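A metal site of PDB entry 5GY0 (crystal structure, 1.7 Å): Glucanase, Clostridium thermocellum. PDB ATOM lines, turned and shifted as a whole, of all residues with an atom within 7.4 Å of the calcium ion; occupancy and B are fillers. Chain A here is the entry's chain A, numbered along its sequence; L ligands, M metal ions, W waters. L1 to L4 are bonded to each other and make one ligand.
OD2 of Asp 246 sits at hydrogen-bond distance from O1 of LG4 L4 (2.7 Å).
An oxygen (O2) of LG2 L2 is in hydrogen-bond range of the indole nitrogen (NE1) of Trp 245.
SG of Cys 244 lies within hydrogen-bond range of O5 of LG3 L3, 3.6 Å away.
Five residues have an atom within 4 Å of the calcium ion: Ser 195, Gly 196, Asp 199, Glu 200 and Asp 246.
The side-chain hydroxyl (OG) of Ser 195 binds the calcium ion (2.3 Å).
The calcium ion is bound by O of Gly 196, 2.3 Å away.
O of Asp 246 binds the calcium ion (2.3 Å).
The calcium ion is bound by water W1, 2.3 Å away.
The calcium ion is bound by the side-chain carboxylate (OE2) of Glu 200 (2.3 Å).
The calcium ion is bound by OD1 of Asp 199.
OD2 of Asp 199 is bound to the calcium ion.
The side-chain carboxylate (OE1) of Glu 200 is bound to the calcium ion (2.6 Å).
The calcium ion has eight donor atoms within binding distance.
Water W1 bridges the side-chain hydroxyl of Ser 193 (2.7 Å) and the side-chain carboxylate of Asp 246 (2.9 Å).
The side-chain carboxylate (OD1) of Asp 246 sits at hydrogen-bond distance from the backbone NH (N) of His 194, 2.9 Å away.
O of Ser 195 is in hydrogen-bond range of ND2 of Asn 229, 3.0 Å away.
The backbone NH (N) of Asp 246 lies close to the side-chain sulfur (SG) of Cys 244 (3.7 Å).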
ATOM      1  N   LEU A  59      23.995  15.422   6.288  1.00  0.00           N
ATOM      2  CA  LEU A  59      22.723  16.084   6.535  1.00  0.00           C
ATOM      3  C   LEU A  59      22.436  17.218   5.552  1.00  0.00           C
ATOM      4  O   LEU A  59      21.413  17.177   4.848  1.00  0.00           O
ATOM      5  CB  LEU A  59      22.559  16.493   8.006  1.00  0.00           C
ATOM      6  CG  LEU A  59      21.233  17.177   8.386  1.00  0.00           C
ATOM      7  CD1 LEU A  59      20.013  16.296   8.066  1.00  0.00           C
ATOM      8  CD2 LEU A  59      21.263  17.513   9.879  1.00  0.00           C
ATOM      9  N   ALA A 143      17.790  12.039  12.167  1.00  0.00           N
ATOM     10  CA  ALA A 143      17.781  13.203  11.285  1.00  0.00           C
ATOM     11  C   ALA A 143      18.604  12.970  10.025  1.00  0.00           C
ATOM     12  O   ALA A 143      18.093  13.121   8.909  1.00  0.00           O
ATOM     13  CB  ALA A 143      18.230  14.487  12.014  1.00  0.00           C
ATOM     14  N   GLN A 147      16.924  12.204   6.393  1.00  0.00           N
ATOM     15  CA  GLN A 147      17.125  13.125   5.292  1.00  0.00           C
ATOM     16  C   GLN A 147      17.682  12.377   4.078  1.00  0.00           C
ATOM     17  O   GLN A 147      17.256  12.616   2.958  1.00  0.00           O
ATOM     18  CB  GLN A 147      18.051  14.281   5.684  1.00  0.00           C
ATOM     19  CG  GLN A 147      18.159  15.352   4.589  1.00  0.00           C
ATOM     20  CD  GLN A 147      16.834  16.023   4.265  1.00  0.00           C
ATOM     21  OE1 GLN A 147      16.380  15.966   3.116  1.00  0.00           O
ATOM     22  NE2 GLN A 147      16.211  16.655   5.264  1.00  0.00           N
ATOM     23  N   ASP A 181      18.847  10.926  17.734  1.00  0.00           N
ATOM     24  CA  ASP A 181      20.067  11.534  17.197  1.00  0.00           C
ATOM     25  C   ASP A 181      21.358  11.265  17.990  1.00  0.00           C
ATOM     26  O   ASP A 181      22.380  11.899  17.711  1.00  0.00           O
ATOM     27  CB  ASP A 181      19.869  13.037  16.996  1.00  0.00           C
ATOM     28  CG  ASP A 181      18.974  13.349  15.804  1.00  0.00           C
ATOM     29  OD1 ASP A 181      19.036  12.640  14.781  1.00  0.00           O
ATOM     30  OD2 ASP A 181      18.194  14.319  15.903  1.00  0.00           O
ATOM     31  N   SER A 192      24.885  20.521  13.782  1.00  0.00           N
ATOM     32  CA  SER A 192      24.170  19.845  14.865  1.00  0.00           C
ATOM     33  C   SER A 192      22.701  19.674  14.541  1.00  0.00           C
ATOM     34  O   SER A 192      22.125  20.486  13.800  1.00  0.00           O
ATOM     35  CB  SER A 192      24.251  20.674  16.150  1.00  0.00           C
ATOM     36  OG  SER A 192      25.584  20.655  16.646  1.00  0.00           O
ATOM     37  N   SER A 193      22.088  18.637  15.103  1.00  0.00           N
ATOM     38  CA  SER A 193      20.644  18.474  14.977  1.00  0.00           C
ATOM     39  C   SER A 193      19.949  19.375  15.997  1.00  0.00           C
ATOM     40  O   SER A 193      19.914  19.058  17.190  1.00  0.00           O
ATOM     41  CB  SER A 193      20.196  17.024  15.163  1.00  0.00           C
ATOM     42  OG  SER A 193      18.791  16.909  15.003  1.00  0.00           O
ATOM     43  N   HIS A 194      19.417  20.483  15.518  1.00  0.00           N
ATOM     44  CA  HIS A 194      18.854  21.497  16.412  1.00  0.00           C
ATOM     45  C   HIS A 194      17.381  21.225  16.684  1.00  0.00           C
ATOM     46  O   HIS A 194      16.926  21.340  17.835  1.00  0.00           O
ATOM     47  CB  HIS A 194      19.016  22.900  15.829  1.00  0.00           C
ATOM     48  CG  HIS A 194      20.439  23.345  15.728  1.00  0.00           C
ATOM     49  ND1 HIS A 194      21.064  24.075  16.709  1.00  0.00           N
ATOM     50  CD2 HIS A 194      21.363  23.170  14.747  1.00  0.00           C
ATOM     51  CE1 HIS A 194      22.310  24.321  16.349  1.00  0.00           C
ATOM     52  NE2 HIS A 194      22.511  23.789  15.159  1.00  0.00           N
ATOM     53  N   SER A 195      16.658  20.884  15.631  1.00  0.00           N
ATOM     54  CA  SER A 195      15.201  20.676  15.699  1.00  0.00           C
ATOM     55  C   SER A 195      14.844  19.277  16.200  1.00  0.00           C
ATOM     56  O   SER A 195      13.676  19.005  16.476  1.00  0.00           O
ATOM     57  CB  SER A 195      14.539  20.941  14.336  1.00  0.00           C
ATOM     58  OG  SER A 195      15.119  20.205  13.255  1.00  0.00           O
ATOM     59  N   GLY A 196      15.815  18.380  16.297  1.00  0.00           N
ATOM     60  CA  GLY A 196      15.490  16.965  16.485  1.00  0.00           C
ATOM     61  C   GLY A 196      15.123  16.310  15.165  1.00  0.00           C
ATOM     62  O   GLY A 196      15.311  16.887  14.095  1.00  0.00           O
ATOM     63  N   PHE A 197      14.565  15.101  15.243  1.00  0.00           N
ATOM     64  CA  PHE A 197      14.444  14.239  14.075  1.00  0.00           C
ATOM     65  C   PHE A 197      13.028  14.007  13.558  1.00  0.00           C
ATOM     66  O   PHE A 197      12.848  13.417  12.492  1.00  0.00           O
ATOM     67  CB  PHE A 197      15.117  12.887  14.346  1.00  0.00           C
ATOM     68  CG  PHE A 197      14.488  12.117  15.495  1.00  0.00           C
ATOM     69  CD1 PHE A 197      13.287  11.458  15.318  1.00  0.00           C
ATOM     70  CD2 PHE A 197      15.072  12.112  16.746  1.00  0.00           C
ATOM     71  CE1 PHE A 197      12.672  10.775  16.371  1.00  0.00           C
ATOM     72  CE2 PHE A 197      14.465  11.448  17.811  1.00  0.00           C
ATOM     73  CZ  PHE A 197      13.278  10.770  17.606  1.00  0.00           C
ATOM     74  N   TRP A 198      12.009  14.420  14.305  1.00  0.00           N
ATOM     75  CA  TRP A 198      10.644  14.140  13.874  1.00  0.00           C
ATOM     76  C   TRP A 198      10.311  14.797  12.547  1.00  0.00           C
ATOM     77  O   TRP A 198       9.577  14.220  11.750  1.00  0.00           O
ATOM     78  CB  TRP A 198       9.621  14.538  14.939  1.00  0.00           C
ATOM     79  CG  TRP A 198       9.773  13.797  16.233  1.00  0.00           C
ATOM     80  CD1 TRP A 198      10.275  14.289  17.395  1.00  0.00           C
ATOM     81  CD2 TRP A 198       9.449  12.422  16.482  1.00  0.00           C
ATOM     82  NE1 TRP A 198      10.262  13.309  18.361  1.00  0.00           N
ATOM     83  CE2 TRP A 198       9.765  12.162  17.830  1.00  0.00           C
ATOM     84  CE3 TRP A 198       8.925  11.385  15.696  1.00  0.00           C
ATOM     85  CZ2 TRP A 198       9.550  10.908  18.417  1.00  0.00           C
ATOM     86  CZ3 TRP A 198       8.715  10.134  16.291  1.00  0.00           C
ATOM     87  CH2 TRP A 198       9.030   9.917  17.635  1.00  0.00           C
ATOM     88  N   ASP A 199      10.858  15.987  12.305  1.00  0.00           N
ATOM     89  CA  ASP A 199      10.676  16.652  11.022  1.00  0.00           C
ATOM     90  C   ASP A 199      11.293  15.862   9.860  1.00  0.00           C
ATOM     91  O   ASP A 199      10.719  15.825   8.773  1.00  0.00           O
ATOM     92  CB  ASP A 199      11.194  18.095  11.086  1.00  0.00           C
ATOM     93  CG  ASP A 199      12.659  18.193  11.494  1.00  0.00           C
ATOM     94  OD1 ASP A 199      13.063  18.131  12.675  1.00  0.00           O
ATOM     95  OD2 ASP A 199      13.495  18.317  10.572  1.00  0.00           O
ATOM     96  N   GLU A 200      12.445  15.231  10.058  1.00  0.00           N
ATOM     97  CA  GLU A 200      13.029  14.401   9.012  1.00  0.00           C
ATOM     98  C   GLU A 200      12.146  13.175   8.746  1.00  0.00           C
ATOM     99  O   GLU A 200      11.976  12.765   7.601  1.00  0.00           O
ATOM    100  CB  GLU A 200      14.470  13.949   9.334  1.00  0.00           C
ATOM    101  CG  GLU A 200      15.535  15.055   9.171  1.00  0.00           C
ATOM    102  CD  GLU A 200      15.584  16.032  10.343  1.00  0.00           C
ATOM    103  OE1 GLU A 200      14.872  15.763  11.338  1.00  0.00           O
ATOM    104  OE2 GLU A 200      16.321  17.051  10.331  1.00  0.00           O
ATOM    105  N   LEU A 201      11.562  12.625   9.802  1.00  0.00           N
ATOM    106  CA  LEU A 201      10.733  11.433   9.600  1.00  0.00           C
ATOM    107  C   LEU A 201       9.472  11.842   8.834  1.00  0.00           C
ATOM    108  O   LEU A 201       9.032  11.142   7.930  1.00  0.00           O
ATOM    109  CB  LEU A 201      10.375  10.740  10.914  1.00  0.00           C
ATOM    110  CG  LEU A 201      11.551  10.167  11.703  1.00  0.00           C
ATOM    111  CD1 LEU A 201      11.001   9.537  12.985  1.00  0.00           C
ATOM    112  CD2 LEU A 201      12.325   9.122  10.891  1.00  0.00           C
ATOM    113  N   ASN A 229       8.120  20.366  16.970  1.00  0.00           N
ATOM    114  CA  ASN A 229       8.292  21.464  17.916  1.00  0.00           C
ATOM    115  C   ASN A 229       7.177  22.491  17.779  1.00  0.00           C
ATOM    116  O   ASN A 229       6.680  22.738  16.680  1.00  0.00           O
ATOM    117  CB  ASN A 229       9.667  22.135  17.773  1.00  0.00           C
ATOM    118  CG  ASN A 229      10.785  21.126  17.863  1.00  0.00           C
ATOM    119  OD1 ASN A 229      10.758  20.254  18.718  1.00  0.00           O
ATOM    120  ND2 ASN A 229      11.759  21.225  16.956  1.00  0.00           N
ATOM    121  N   CYS A 244      14.957  24.249   5.812  1.00  0.00           N
ATOM    122  CA  CYS A 244      16.423  24.286   5.715  1.00  0.00           C
ATOM    123  C   CYS A 244      16.989  22.907   6.007  1.00  0.00           C
ATOM    124  O   CYS A 244      16.261  21.979   6.362  1.00  0.00           O
ATOM    125  CB  CYS A 244      17.025  25.333   6.675  1.00  0.00           C
ATOM    126  SG  CYS A 244      16.694  24.916   8.400  1.00  0.00           S
ATOM    127  N   TRP A 245      18.298  22.793   5.888  1.00  0.00           N
ATOM    128  CA  TRP A 245      19.013  21.537   6.129  1.00  0.00           C
ATOM    129  C   TRP A 245      18.665  20.863   7.455  1.00  0.00           C
ATOM    130  O   TRP A 245      18.747  19.635   7.564  1.00  0.00           O
ATOM    131  CB  TRP A 245      20.526  21.756   6.017  1.00  0.00           C
ATOM    132  CG  TRP A 245      21.037  22.692   7.086  1.00  0.00           C
ATOM    133  CD1 TRP A 245      21.250  24.043   6.976  1.00  0.00           C
ATOM    134  CD2 TRP A 245      21.419  22.343   8.422  1.00  0.00           C
ATOM    135  NE1 TRP A 245      21.714  24.556   8.182  1.00  0.00           N
ATOM    136  CE2 TRP A 245      21.838  23.519   9.074  1.00  0.00           C
ATOM    137  CE3 TRP A 245      21.464  21.123   9.134  1.00  0.00           C
ATOM    138  CZ2 TRP A 245      22.273  23.532  10.397  1.00  0.00           C
ATOM    139  CZ3 TRP A 245      21.888  21.136  10.465  1.00  0.00           C
ATOM    140  CH2 TRP A 245      22.273  22.333  11.080  1.00  0.00           C
ATOM    141  N   ASP A 246      18.333  21.648   8.482  1.00  0.00           N
ATOM    142  CA  ASP A 246      18.026  21.116   9.812  1.00  0.00           C
ATOM    143  C   ASP A 246      16.566  20.724   9.994  1.00  0.00           C
ATOM    144  O   ASP A 246      16.230  19.922  10.885  1.00  0.00           O
ATOM    145  CB  ASP A 246      18.336  22.172  10.871  1.00  0.00           C
ATOM    146  CG  ASP A 246      18.191  21.621  12.274  1.00  0.00           C
ATOM    147  OD1 ASP A 246      19.001  20.730  12.624  1.00  0.00           O
ATOM    148  OD2 ASP A 246      17.282  22.077  13.004  1.00  0.00           O
ATOM    149  N   ASP A 247      15.690  21.316   9.179  1.00  0.00           N
ATOM    150  CA  ASP A 247      14.268  21.210   9.453  1.00  0.00           C
ATOM    151  C   ASP A 247      13.440  21.423   8.188  1.00  0.00           C
ATOM    152  O   ASP A 247      13.268  22.553   7.731  1.00  0.00           O
ATOM    153  CB  ASP A 247      13.908  22.282  10.489  1.00  0.00           C
ATOM    154  CG  ASP A 247      12.519  22.103  11.064  1.00  0.00           C
ATOM    155  OD1 ASP A 247      11.723  21.289  10.547  1.00  0.00           O
ATOM    156  OD2 ASP A 247      12.226  22.827  12.037  1.00  0.00           O
ATOM    157  N   CYS A 248      12.888  20.331   7.674  1.00  0.00           N
ATOM    158  CA  CYS A 248      12.084  20.364   6.465  1.00  0.00           C
ATOM    159  C   CYS A 248      10.588  20.206   6.760  1.00  0.00           C
ATOM    160  O   CYS A 248       9.831  19.874   5.843  1.00  0.00           O
ATOM    161  CB  CYS A 248      12.530  19.244   5.529  1.00  0.00           C
ATOM    162  SG  CYS A 248      14.147  19.547   4.782  1.00  0.00           S
ATOM    163  N   HIS A 249      10.142  20.420   7.993  1.00  0.00           N
ATOM    164  CA  HIS A 249       8.704  20.254   8.224  1.00  0.00           C
ATOM    165  C   HIS A 249       7.860  21.278   7.472  1.00  0.00           C
ATOM    166  O   HIS A 249       6.724  20.953   7.090  1.00  0.00           O
ATOM    167  CB  HIS A 249       8.288  20.162   9.700  1.00  0.00           C
ATOM    168  CG  HIS A 249       8.153  21.472  10.418  1.00  0.00           C
ATOM    169  ND1 HIS A 249       9.203  22.035  11.113  1.00  0.00           N
ATOM    170  CD2 HIS A 249       7.081  22.268  10.651  1.00  0.00           C
ATOM    171  CE1 HIS A 249       8.788  23.146  11.709  1.00  0.00           C
ATOM    172  NE2 HIS A 249       7.503  23.295  11.463  1.00  0.00           N
HETATM  173  C1  LIG L   1      30.598  25.293   8.237  1.00  0.00           C
HETATM  174  C2  LIG L   1      29.095  25.245   8.531  1.00  0.00           C
HETATM  175  C3  LIG L   1      28.406  26.539   8.115  1.00  0.00           C
HETATM  176  C4  LIG L   1      28.788  26.849   6.667  1.00  0.00           C
HETATM  177  C5  LIG L   1      28.010  28.024   6.066  1.00  0.00           C
HETATM  178  C6  LIG L   1      30.895  25.839   6.831  1.00  0.00           C
HETATM  179  O1  LIG L   1      32.293  26.073   6.628  1.00  0.00           O
HETATM  180  O2  LIG L   1      31.118  23.970   8.436  1.00  0.00           O
HETATM  181  O3  LIG L   1      28.809  24.953   9.905  1.00  0.00           O
HETATM  182  O4  LIG L   1      26.989  26.386   8.275  1.00  0.00           O
HETATM  183  O5  LIG L   1      30.203  27.071   6.649  1.00  0.00           O
HETATM  184  O6  LIG L   1      28.209  29.098   6.990  1.00  0.00           O
HETATM  185  C1  LG2 L   2      24.781  26.913   8.644  1.00  0.00           C
HETATM  186  C2  LG2 L   2      23.802  27.574   9.612  1.00  0.00           C
HETATM  187  C3  LG2 L   2      24.054  27.065  11.039  1.00  0.00           C
HETATM  188  C4  LG2 L   2      25.527  27.223  11.418  1.00  0.00           C
HETATM  189  C5  LG2 L   2      25.886  26.548  12.747  1.00  0.00           C
HETATM  190  C6  LG2 L   2      26.196  27.225   9.131  1.00  0.00           C
HETATM  191  O1  LG2 L   2      24.572  27.419   7.316  1.00  0.00           O
HETATM  192  O2  LG2 L   2      22.481  27.204   9.237  1.00  0.00           O
HETATM  193  O3  LG2 L   2      23.155  27.764  11.910  1.00  0.00           O
HETATM  194  O4  LG2 L   2      26.355  26.624  10.416  1.00  0.00           O
HETATM  195  O5  LG2 L   2      25.575  25.131  12.707  1.00  0.00           O
HETATM  196  C1  LG3 L   3      21.757  27.712  13.818  1.00  0.00           C
HETATM  197  C2  LG3 L   3      20.606  26.937  14.463  1.00  0.00           C
HETATM  198  C3  LG3 L   3      19.567  26.629  13.400  1.00  0.00           C
HETATM  199  C4  LG3 L   3      20.188  25.949  12.178  1.00  0.00           C
HETATM  200  C5  LG3 L   3      19.170  25.691  11.068  1.00  0.00           C
HETATM  201  C6  LG3 L   3      22.277  26.902  12.641  1.00  0.00           C
HETATM  202  O1  LG3 L   3      22.800  27.944  14.766  1.00  0.00           O
HETATM  203  O2  LG3 L   3      20.021  27.737  15.509  1.00  0.00           O
HETATM  204  O3  LG3 L   3      18.529  25.797  13.937  1.00  0.00           O
HETATM  205  O4  LG3 L   3      21.228  26.774  11.669  1.00  0.00           O
HETATM  206  O5  LG3 L   3      18.636  26.926  10.593  1.00  0.00           O
HETATM  207  C1  LG4 L   4      16.164  25.204  14.040  1.00  0.00           C
HETATM  208  C2  LG4 L   4      14.772  25.776  14.330  1.00  0.00           C
HETATM  209  C3  LG4 L   4      14.853  26.743  15.496  1.00  0.00           C
HETATM  210  C4  LG4 L   4      15.891  27.817  15.211  1.00  0.00           C
HETATM  211  C5  LG4 L   4      15.980  28.907  16.284  1.00  0.00           C
HETATM  212  C6  LG4 L   4      17.193  26.320  13.911  1.00  0.00           C
HETATM  213  O1  LG4 L   4      16.107  24.450  12.823  1.00  0.00           O
HETATM  214  O2  LG4 L   4      13.901  24.683  14.659  1.00  0.00           O
HETATM  215  O3  LG4 L   4      13.560  27.312  15.744  1.00  0.00           O
HETATM  216  O4  LG4 L   4      17.166  27.187  15.052  1.00  0.00           O
HETATM  217  O5  LG4 L   4      16.468  28.362  17.521  1.00  0.00           O
HETATM  218 CA    CA M   1      15.352  18.170  12.151  1.00  0.00          CA
HETATM  219  O   HOH W   1      17.530  18.280  13.004  1.00  0.00           O
